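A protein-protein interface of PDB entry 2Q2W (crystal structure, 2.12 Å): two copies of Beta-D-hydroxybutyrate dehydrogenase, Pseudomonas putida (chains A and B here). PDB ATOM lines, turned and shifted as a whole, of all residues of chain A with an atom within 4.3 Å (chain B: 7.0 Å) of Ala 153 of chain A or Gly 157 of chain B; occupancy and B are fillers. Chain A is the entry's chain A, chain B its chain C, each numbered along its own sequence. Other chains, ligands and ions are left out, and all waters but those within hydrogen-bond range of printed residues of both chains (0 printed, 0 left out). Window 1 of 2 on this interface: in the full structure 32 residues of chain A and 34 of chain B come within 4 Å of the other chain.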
ATOM      1  N   TRP A 103      12.950 -24.399  10.128  1.00  0.00           N
ATOM      2  CA  TRP A 103      11.620 -24.237  10.755  1.00  0.00           C
ATOM      3  C   TRP A 103      10.596 -25.284  10.168  1.00  0.00           C
ATOM      4  O   TRP A 103       9.953 -26.005  10.928  1.00  0.00           O
ATOM      5  CB  TRP A 103      11.078 -22.764  10.746  1.00  0.00           C
ATOM      6  CG  TRP A 103       9.517 -22.699  11.141  1.00  0.00           C
ATOM      7  CD1 TRP A 103       8.432 -22.943  10.303  1.00  0.00           C
ATOM      8  CD2 TRP A 103       8.947 -22.416  12.442  1.00  0.00           C
ATOM      9  NE1 TRP A 103       7.232 -22.836  10.993  1.00  0.00           N
ATOM     10  CE2 TRP A 103       7.508 -22.535  12.308  1.00  0.00           C
ATOM     11  CE3 TRP A 103       9.502 -22.081  13.699  1.00  0.00           C
ATOM     12  CZ2 TRP A 103       6.618 -22.300  13.373  1.00  0.00           C
ATOM     13  CZ3 TRP A 103       8.603 -21.861  14.804  1.00  0.00           C
ATOM     14  CH2 TRP A 103       7.153 -22.022  14.626  1.00  0.00           C
ATOM     15  N   ALA A 149      13.370 -21.814  18.946  1.00  0.00           N
ATOM     16  CA  ALA A 149      12.013 -21.465  18.566  1.00  0.00           C
ATOM     17  C   ALA A 149      11.214 -22.615  17.909  1.00  0.00           C
ATOM     18  O   ALA A 149      10.098 -22.933  18.334  1.00  0.00           O
ATOM     19  CB  ALA A 149      12.092 -20.242  17.652  1.00  0.00           C
ATOM     20  N   ALA A 150      11.763 -23.257  16.870  1.00  0.00           N
ATOM     21  CA  ALA A 150      11.032 -24.321  16.191  1.00  0.00           C
ATOM     22  C   ALA A 150      10.750 -25.520  17.069  1.00  0.00           C
ATOM     23  O   ALA A 150       9.640 -26.114  17.076  1.00  0.00           O
ATOM     24  CB  ALA A 150      11.797 -24.758  14.960  1.00  0.00           C
ATOM     25  N   TYR A 151      11.741 -25.929  17.813  1.00  0.00           N
ATOM     26  CA  TYR A 151      11.604 -27.138  18.597  1.00  0.00           C
ATOM     27  C   TYR A 151      10.609 -26.966  19.745  1.00  0.00           C
ATOM     28  O   TYR A 151       9.768 -27.863  20.000  1.00  0.00           O
ATOM     29  CB  TYR A 151      12.995 -27.526  19.122  1.00  0.00           C
ATOM     30  CG  TYR A 151      13.033 -28.899  19.765  1.00  0.00           C
ATOM     31  CD1 TYR A 151      12.972 -29.053  21.117  1.00  0.00           C
ATOM     32  CD2 TYR A 151      13.109 -30.041  18.996  1.00  0.00           C
ATOM     33  CE1 TYR A 151      13.075 -30.338  21.725  1.00  0.00           C
ATOM     34  CE2 TYR A 151      13.187 -31.305  19.586  1.00  0.00           C
ATOM     35  CZ  TYR A 151      13.181 -31.440  20.956  1.00  0.00           C
ATOM     36  OH  TYR A 151      13.226 -32.715  21.540  1.00  0.00           O
ATOM     37  N   VAL A 152      10.725 -25.808  20.423  1.00  0.00           N
ATOM     38  CA  VAL A 152       9.816 -25.433  21.469  1.00  0.00           C
ATOM     39  C   VAL A 152       8.369 -25.316  20.919  1.00  0.00           C
ATOM     40  O   VAL A 152       7.500 -25.887  21.488  1.00  0.00           O
ATOM     41  CB  VAL A 152      10.331 -24.185  22.176  1.00  0.00           C
ATOM     42  CG1 VAL A 152       9.308 -23.641  23.092  1.00  0.00           C
ATOM     43  CG2 VAL A 152      11.712 -24.494  22.948  1.00  0.00           C
ATOM     44  N   ALA A 153       8.158 -24.664  19.754  1.00  0.00           N
ATOM     45  CA  ALA A 153       6.829 -24.540  19.156  1.00  0.00           C
ATOM     46  C   ALA A 153       6.241 -25.950  18.848  1.00  0.00           C
ATOM     47  O   ALA A 153       5.058 -26.229  19.216  1.00  0.00           O
ATOM     48  CB  ALA A 153       6.860 -23.655  17.890  1.00  0.00           C
ATOM     49  N   ALA A 154       7.069 -26.823  18.233  1.00  0.00           N
ATOM     50  CA  ALA A 154       6.661 -28.174  17.827  1.00  0.00           C
ATOM     51  C   ALA A 154       6.251 -29.070  19.028  1.00  0.00           C
ATOM     52  O   ALA A 154       5.165 -29.677  19.045  1.00  0.00           O
ATOM     53  CB  ALA A 154       7.794 -28.864  16.968  1.00  0.00           C
ATOM     54  N   LYS A 155       7.091 -29.056  20.049  1.00  0.00           N
ATOM     55  CA  LYS A 155       6.882 -29.936  21.207  1.00  0.00           C
ATOM     56  C   LYS A 155       5.740 -29.444  22.086  1.00  0.00           C
ATOM     57  O   LYS A 155       5.052 -30.256  22.711  1.00  0.00           O
ATOM     58  CB  LYS A 155       8.168 -30.100  22.035  1.00  0.00           C
ATOM     59  CG  LYS A 155       9.344 -30.795  21.314  1.00  0.00           C
ATOM     60  CD  LYS A 155       8.853 -32.169  20.827  1.00  0.00           C
ATOM     61  CE  LYS A 155       9.976 -33.206  20.788  1.00  0.00           C
ATOM     62  NZ  LYS A 155       9.699 -34.385  19.895  1.00  0.00           N
ATOM     63  N   HIS A 156       5.526 -28.119  22.113  1.00  0.00           N
ATOM     64  CA  HIS A 156       4.354 -27.551  22.742  1.00  0.00           C
ATOM     65  C   HIS A 156       3.106 -27.954  21.951  1.00  0.00           C
ATOM     66  O   HIS A 156       2.122 -28.366  22.507  1.00  0.00           O
ATOM     67  CB  HIS A 156       4.423 -25.990  22.729  1.00  0.00           C
ATOM     68  CG  HIS A 156       4.962 -25.375  23.977  1.00  0.00           C
ATOM     69  ND1 HIS A 156       6.315 -25.377  24.283  1.00  0.00           N
ATOM     70  CD2 HIS A 156       4.349 -24.693  24.968  1.00  0.00           C
ATOM     71  CE1 HIS A 156       6.501 -24.748  25.433  1.00  0.00           C
ATOM     72  NE2 HIS A 156       5.321 -24.344  25.876  1.00  0.00           N
ATOM     73  N   GLY A 157       3.170 -27.874  20.635  1.00  0.00           N
ATOM     74  CA  GLY A 157       2.100 -28.388  19.811  1.00  0.00           C
ATOM     75  C   GLY A 157       1.786 -29.837  20.100  1.00  0.00           C
ATOM     76  O   GLY A 157       0.590 -30.241  20.120  1.00  0.00           O
ATOM     77  N   ASN B 110      -1.891 -20.359  11.830  1.00  0.00           N
ATOM     78  CA  ASN B 110      -2.001 -20.081  13.300  1.00  0.00           C
ATOM     79  C   ASN B 110      -0.684 -20.160  13.960  1.00  0.00           C
ATOM     80  O   ASN B 110      -0.511 -19.558  15.017  1.00  0.00           O
ATOM     81  CB  ASN B 110      -3.044 -20.953  14.019  1.00  0.00           C
ATOM     82  CG  ASN B 110      -4.474 -20.610  13.598  1.00  0.00           C
ATOM     83  OD1 ASN B 110      -5.204 -19.968  14.321  1.00  0.00           O
ATOM     84  ND2 ASN B 110      -4.813 -20.930  12.398  1.00  0.00           N
ATOM     85  N   LEU B 111       0.267 -20.850  13.338  1.00  0.00           N
ATOM     86  CA  LEU B 111       1.534 -21.054  13.991  1.00  0.00           C
ATOM     87  C   LEU B 111       2.688 -20.500  13.203  1.00  0.00           C
ATOM     88  O   LEU B 111       3.379 -19.602  13.705  1.00  0.00           O
ATOM     89  CB  LEU B 111       1.764 -22.550  14.330  1.00  0.00           C
ATOM     90  CG  LEU B 111       3.150 -22.811  14.940  1.00  0.00           C
ATOM     91  CD1 LEU B 111       3.396 -22.016  16.244  1.00  0.00           C
ATOM     92  CD2 LEU B 111       3.374 -24.307  15.182  1.00  0.00           C
ATOM     93  N   PHE B 115       5.812 -17.143  13.683  1.00  0.00           N
ATOM     94  CA  PHE B 115       7.267 -17.196  13.501  1.00  0.00           C
ATOM     95  C   PHE B 115       7.701 -16.320  12.295  1.00  0.00           C
ATOM     96  O   PHE B 115       8.686 -15.545  12.419  1.00  0.00           O
ATOM     97  CB  PHE B 115       7.704 -18.653  13.284  1.00  0.00           C
ATOM     98  CG  PHE B 115       9.056 -18.794  12.667  1.00  0.00           C
ATOM     99  CD1 PHE B 115      10.208 -18.634  13.454  1.00  0.00           C
ATOM    100  CD2 PHE B 115       9.190 -19.106  11.285  1.00  0.00           C
ATOM    101  CE1 PHE B 115      11.503 -18.799  12.875  1.00  0.00           C
ATOM    102  CE2 PHE B 115      10.459 -19.247  10.710  1.00  0.00           C
ATOM    103  CZ  PHE B 115      11.625 -19.090  11.503  1.00  0.00           C
ATOM    104  N   HIS B 140      -6.837 -22.384  24.043  1.00  0.00           N
ATOM    105  CA  HIS B 140      -6.450 -23.605  23.339  1.00  0.00           C
ATOM    106  C   HIS B 140      -4.948 -23.652  23.102  1.00  0.00           C
ATOM    107  O   HIS B 140      -4.423 -24.613  22.576  1.00  0.00           O
ATOM    108  CB  HIS B 140      -7.291 -23.722  22.093  1.00  0.00           C
ATOM    109  CG  HIS B 140      -8.720 -24.140  22.392  1.00  0.00           C
ATOM    110  ND1 HIS B 140      -9.027 -25.174  23.263  1.00  0.00           N
ATOM    111  CD2 HIS B 140      -9.903 -23.670  21.929  1.00  0.00           C
ATOM    112  CE1 HIS B 140     -10.350 -25.282  23.353  1.00  0.00           C
ATOM    113  NE2 HIS B 140     -10.900 -24.362  22.567  1.00  0.00           N
ATOM    114  N   GLY B 141      -4.261 -22.611  23.585  1.00  0.00           N
ATOM    115  CA  GLY B 141      -2.826 -22.678  23.681  1.00  0.00           C
ATOM    116  C   GLY B 141      -2.386 -23.246  25.023  1.00  0.00           C
ATOM    117  O   GLY B 141      -1.185 -23.403  25.248  1.00  0.00           O
ATOM    118  N   TYR B 151      -6.009 -26.750  15.679  1.00  0.00           N
ATOM    119  CA  TYR B 151      -6.017 -25.479  16.378  1.00  0.00           C
ATOM    120  C   TYR B 151      -5.300 -25.475  17.755  1.00  0.00           C
ATOM    121  O   TYR B 151      -4.520 -24.533  18.078  1.00  0.00           O
ATOM    122  CB  TYR B 151      -7.484 -25.000  16.479  1.00  0.00           C
ATOM    123  CG  TYR B 151      -7.663 -23.567  16.962  1.00  0.00           C
ATOM    124  CD1 TYR B 151      -7.984 -23.289  18.286  1.00  0.00           C
ATOM    125  CD2 TYR B 151      -7.583 -22.487  16.061  1.00  0.00           C
ATOM    126  CE1 TYR B 151      -8.172 -21.980  18.724  1.00  0.00           C
ATOM    127  CE2 TYR B 151      -7.781 -21.174  16.496  1.00  0.00           C
ATOM    128  CZ  TYR B 151      -8.068 -20.938  17.804  1.00  0.00           C
ATOM    129  OH  TYR B 151      -8.262 -19.634  18.193  1.00  0.00           O
ATOM    130  N   VAL B 152      -5.585 -26.499  18.596  1.00  0.00           N
ATOM    131  CA  VAL B 152      -4.948 -26.584  19.893  1.00  0.00           C
ATOM    132  C   VAL B 152      -3.452 -26.807  19.704  1.00  0.00           C
ATOM    133  O   VAL B 152      -2.681 -26.226  20.393  1.00  0.00           O
ATOM    134  CB  VAL B 152      -5.570 -27.751  20.701  1.00  0.00           C
ATOM    135  CG1 VAL B 152      -4.728 -28.181  21.866  1.00  0.00           C
ATOM    136  CG2 VAL B 152      -6.905 -27.371  21.152  1.00  0.00           C
ATOM    137  N   ALA B 153      -3.070 -27.653  18.737  1.00  0.00           N
ATOM    138  CA  ALA B 153      -1.682 -27.872  18.457  1.00  0.00           C
ATOM    139  C   ALA B 153      -0.994 -26.546  18.046  1.00  0.00           C
ATOM    140  O   ALA B 153       0.067 -26.194  18.623  1.00  0.00           O
ATOM    141  CB  ALA B 153      -1.520 -28.985  17.388  1.00  0.00           C
ATOM    142  N   ALA B 154      -1.590 -25.815  17.068  1.00  0.00           N
ATOM    143  CA  ALA B 154      -0.975 -24.515  16.610  1.00  0.00           C
ATOM    144  C   ALA B 154      -0.882 -23.509  17.746  1.00  0.00           C
ATOM    145  O   ALA B 154       0.131 -22.845  17.901  1.00  0.00           O
ATOM    146  CB  ALA B 154      -1.830 -23.881  15.464  1.00  0.00           C
ATOM    147  N   LYS B 155      -1.983 -23.356  18.507  1.00  0.00           N
ATOM    148  CA  LYS B 155      -2.056 -22.317  19.615  1.00  0.00           C
ATOM    149  C   LYS B 155      -1.066 -22.603  20.780  1.00  0.00           C
ATOM    150  O   LYS B 155      -0.364 -21.716  21.318  1.00  0.00           O
ATOM    151  CB  LYS B 155      -3.513 -22.138  20.068  1.00  0.00           C
ATOM    152  CG  LYS B 155      -4.435 -21.473  19.012  1.00  0.00           C
ATOM    153  CD  LYS B 155      -3.831 -20.141  18.518  1.00  0.00           C
ATOM    154  CE  LYS B 155      -4.958 -19.219  17.896  1.00  0.00           C
ATOM    155  NZ  LYS B 155      -4.507 -17.978  17.050  1.00  0.00           N
ATOM    156  N   HIS B 156      -0.922 -23.873  21.105  1.00  0.00           N
ATOM    157  CA  HIS B 156       0.158 -24.320  21.964  1.00  0.00           C
ATOM    158  C   HIS B 156       1.538 -23.945  21.474  1.00  0.00           C
ATOM    159  O   HIS B 156       2.361 -23.404  22.261  1.00  0.00           O
ATOM    160  CB  HIS B 156       0.077 -25.870  22.229  1.00  0.00           C
ATOM    161  CG  HIS B 156      -0.846 -26.237  23.366  1.00  0.00           C
ATOM    162  ND1 HIS B 156      -2.218 -26.105  23.269  1.00  0.00           N
ATOM    163  CD2 HIS B 156      -0.612 -26.804  24.579  1.00  0.00           C
ATOM    164  CE1 HIS B 156      -2.777 -26.488  24.411  1.00  0.00           C
ATOM    165  NE2 HIS B 156      -1.838 -26.919  25.212  1.00  0.00           N
ATOM    166  N   GLY B 157       1.786 -24.207  20.175  1.00  0.00           N
ATOM    167  CA  GLY B 157       3.055 -23.848  19.511  1.00  0.00           C
ATOM    168  C   GLY B 157       3.350 -22.357  19.660  1.00  0.00           C
ATOM    169  O   GLY B 157       4.485 -21.963  19.885  1.00  0.00           O
ATOM    170  N   VAL B 158       2.320 -21.549  19.530  1.00  0.00           N
ATOM    171  CA  VAL B 158       2.411 -20.075  19.736  1.00  0.00           C
ATOM    172  C   VAL B 158       2.806 -19.706  21.136  1.00  0.00           C
ATOM    173  O   VAL B 158       3.716 -18.881  21.292  1.00  0.00           O
ATOM    174  CB  VAL B 158       1.083 -19.310  19.374  1.00  0.00           C
ATOM    175  CG1 VAL B 158       1.140 -17.798  19.857  1.00  0.00           C
ATOM    176  CG2 VAL B 158       0.800 -19.413  17.838  1.00  0.00           C
ATOM    177  N   VAL B 159       2.140 -20.314  22.123  1.00  0.00           N
ATOM    178  CA  VAL B 159       2.468 -20.111  23.559  1.00  0.00           C
ATOM    179  C   VAL B 159       3.961 -20.439  23.780  1.00  0.00           C
ATOM    180  O   VAL B 159       4.703 -19.726  24.507  1.00  0.00           O
ATOM    181  CB  VAL B 159       1.500 -20.890  24.528  1.00  0.00           C
ATOM    182  CG1 VAL B 159       1.983 -20.864  26.059  1.00  0.00           C
ATOM    183  CG2 VAL B 159       0.068 -20.293  24.421  1.00  0.00           C
ATOM    184  N   GLY B 160       4.440 -21.486  23.095  1.00  0.00           N
ATOM    185  CA  GLY B 160       5.820 -21.869  23.336  1.00  0.00           C
ATOM    186  C   GLY B 160       6.822 -21.020  22.611  1.00  0.00           C
ATOM    187  O   GLY B 160       7.822 -20.652  23.169  1.00  0.00           O
ATOM    188  N   LEU B 161       6.548 -20.716  21.347  1.00  0.00           N
ATOM    189  CA  LEU B 161       7.298 -19.692  20.615  1.00  0.00           C
ATOM    190  C   LEU B 161       7.316 -18.342  21.368  1.00  0.00           C
ATOM    191  O   LEU B 161       8.314 -17.704  21.437  1.00  0.00           O
ATOM    192  CB  LEU B 161       6.687 -19.518  19.202  1.00  0.00           C
ATOM    193  CG  LEU B 161       7.341 -18.466  18.277  1.00  0.00           C
ATOM    194  CD1 LEU B 161       8.913 -18.668  18.224  1.00  0.00           C
ATOM    195  CD2 LEU B 161       6.615 -18.581  16.894  1.00  0.00           C
ATOM    196  N   THR B 162       6.204 -17.918  21.954  1.00  0.00           N
ATOM    197  CA  THR B 162       6.237 -16.724  22.814  1.00  0.00           C
ATOM    198  C   THR B 162       7.381 -16.708  23.899  1.00  0.00           C
ATOM    199  O   THR B 162       8.001 -15.670  24.119  1.00  0.00           O
ATOM    200  CB  THR B 162       4.853 -16.447  23.450  1.00  0.00           C
ATOM    201  OG1 THR B 162       3.868 -16.348  22.410  1.00  0.00           O
ATOM    202  CG2 THR B 162       4.826 -15.172  24.236  1.00  0.00           C
ATOM    203  N   LYS B 163       7.577 -17.851  24.581  1.00  0.00           N
ATOM    204  CA  LYS B 163       8.480 -17.991  25.663  1.00  0.00           C
ATOM    205  C   LYS B 163       9.865 -17.846  25.089  1.00  0.00           C
ATOM    206  O   LYS B 163      10.617 -17.059  25.614  1.00  0.00           O
ATOM    207  CB  LYS B 163       8.369 -19.377  26.307  1.00  0.00           C
ATOM    208  CG  LYS B 163       6.957 -19.597  26.958  1.00  0.00           C
ATOM    209  CD  LYS B 163       6.839 -20.937  27.726  1.00  0.00           C
ATOM    210  CE  LYS B 163       5.355 -21.311  27.812  1.00  0.00           C
ATOM    211  NZ  LYS B 163       5.091 -22.796  28.154  1.00  0.00           N
ATOM    212  N   VAL B 164      10.187 -18.590  24.007  1.00  0.00           N
ATOM    213  CA  VAL B 164      11.461 -18.521  23.390  1.00  0.00           C
ATOM    214  C   VAL B 164      11.778 -17.057  22.988  1.00  0.00           C
ATOM    215  O   VAL B 164      12.910 -16.581  23.201  1.00  0.00           O
ATOM    216  CB  VAL B 164      11.545 -19.427  22.131  1.00  0.00           C
ATOM    217  CG1 VAL B 164      12.813 -19.160  21.330  1.00  0.00           C
ATOM    218  CG2 VAL B 164      11.452 -20.850  22.504  1.00  0.00           C
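A ring nitrogen (NE2) of His 156 of chain A is in hydrogen-bond range of the side-chain amino group (NZ) of Lys 163 of chain B.
Of the 19 printed residues of chain B, 9 touch a printed residue of chain A.
Hydrophobic or aromatic side chains of chain B that line the printed part of chain A: Leu 111, Phe 115, Ala 153, His 156, Leu 161 and Val 164.
Along chain B the printed residues that touch a printed residue of chain A span positions 111 to 164.
Of the 10 printed residues of chain A, 6 touch a printed residue of chain B.
Printed residues of chain A that touch a printed residue of chain B: Trp 103, Ala 149, Val 152, Ala 153, His 156 and Gly 157.
Among the printed residues, no Asp or Glu carboxylate lies within 4 Å of a Lys or Arg side-chain nitrogen of the other chain.
Ala 153 of chain A touches Gly 157 of chain B, and with the chains exchanged Gly 157 of chain A touches Ala 153 of chain B.
His 156 of chain A touches its own counterpart, His 156 of chain B.
Gly 157 of chain B touches its own counterpart, Gly 157 of chain A.
Among the printed residues, pairs that only touch across the chains: Trp 103 of chain A with Leu 111 of chain B, Trp 103 of chain A with Phe 115 of chain B, Ala 149 of chain A with Leu 161 of chain B, Ala 149 of chain A with Val 164 of chain B, Val 152 of chain A with Gly 160 of chain B, Val 152 of chain A with Val 164 of chain B, Ala 153 of chain A with Gly 157 of chain B, His 156 of chain A with His 156 of chain B, His 156 of chain A with Gly 160 of chain B, Gly 157 of chain A with Ala 153 of chain B and Gly 157 of chain A with Gly 157 of chain B.
The backbone carbonyl oxygen of Val 152 of chain A lies within hydrogen-bond range of a ring nitrogen (ND1) of His 156 of chain A (3.1 Å).
The backbone carbonyl oxygen of His 140 of chain B is in hydrogen-bond range of a ring nitrogen (ND1) of His 156 of chain B (2.8 Å).
A ring nitrogen (ND1) of His 156 of chain B is in hydrogen-bond range of the backbone carbonyl oxygen of Val 152 of chain B, 2.9 Å away.
Ala 153 of chain A touches just one residue of chain B: Gly 157 (3.1 Å).
Asn 110 of chain B touches none of the printed residues of chain A.
Of the printed residues of chain A, Ala 153 of chain B touches Gly 157.
Printed residues of chain A within 4 Å of His 156 of chain B: His 156 (3.2 Å).
Gly 157 of chain B touches just these residues of chain A: Ala 153 (3.1 Å) and Gly 157 (3.9 Å).
Printed residues of chain A within 4 Å of Leu 161 of chain B: Ala 149.
Of the printed residues of chain A, Lys 163 of chain B touches His 156 (2.8 Å).
The nearest printed residue of chain A that does not touch Lys 163 of chain B is Val 152 of chain A (5.4 Å).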
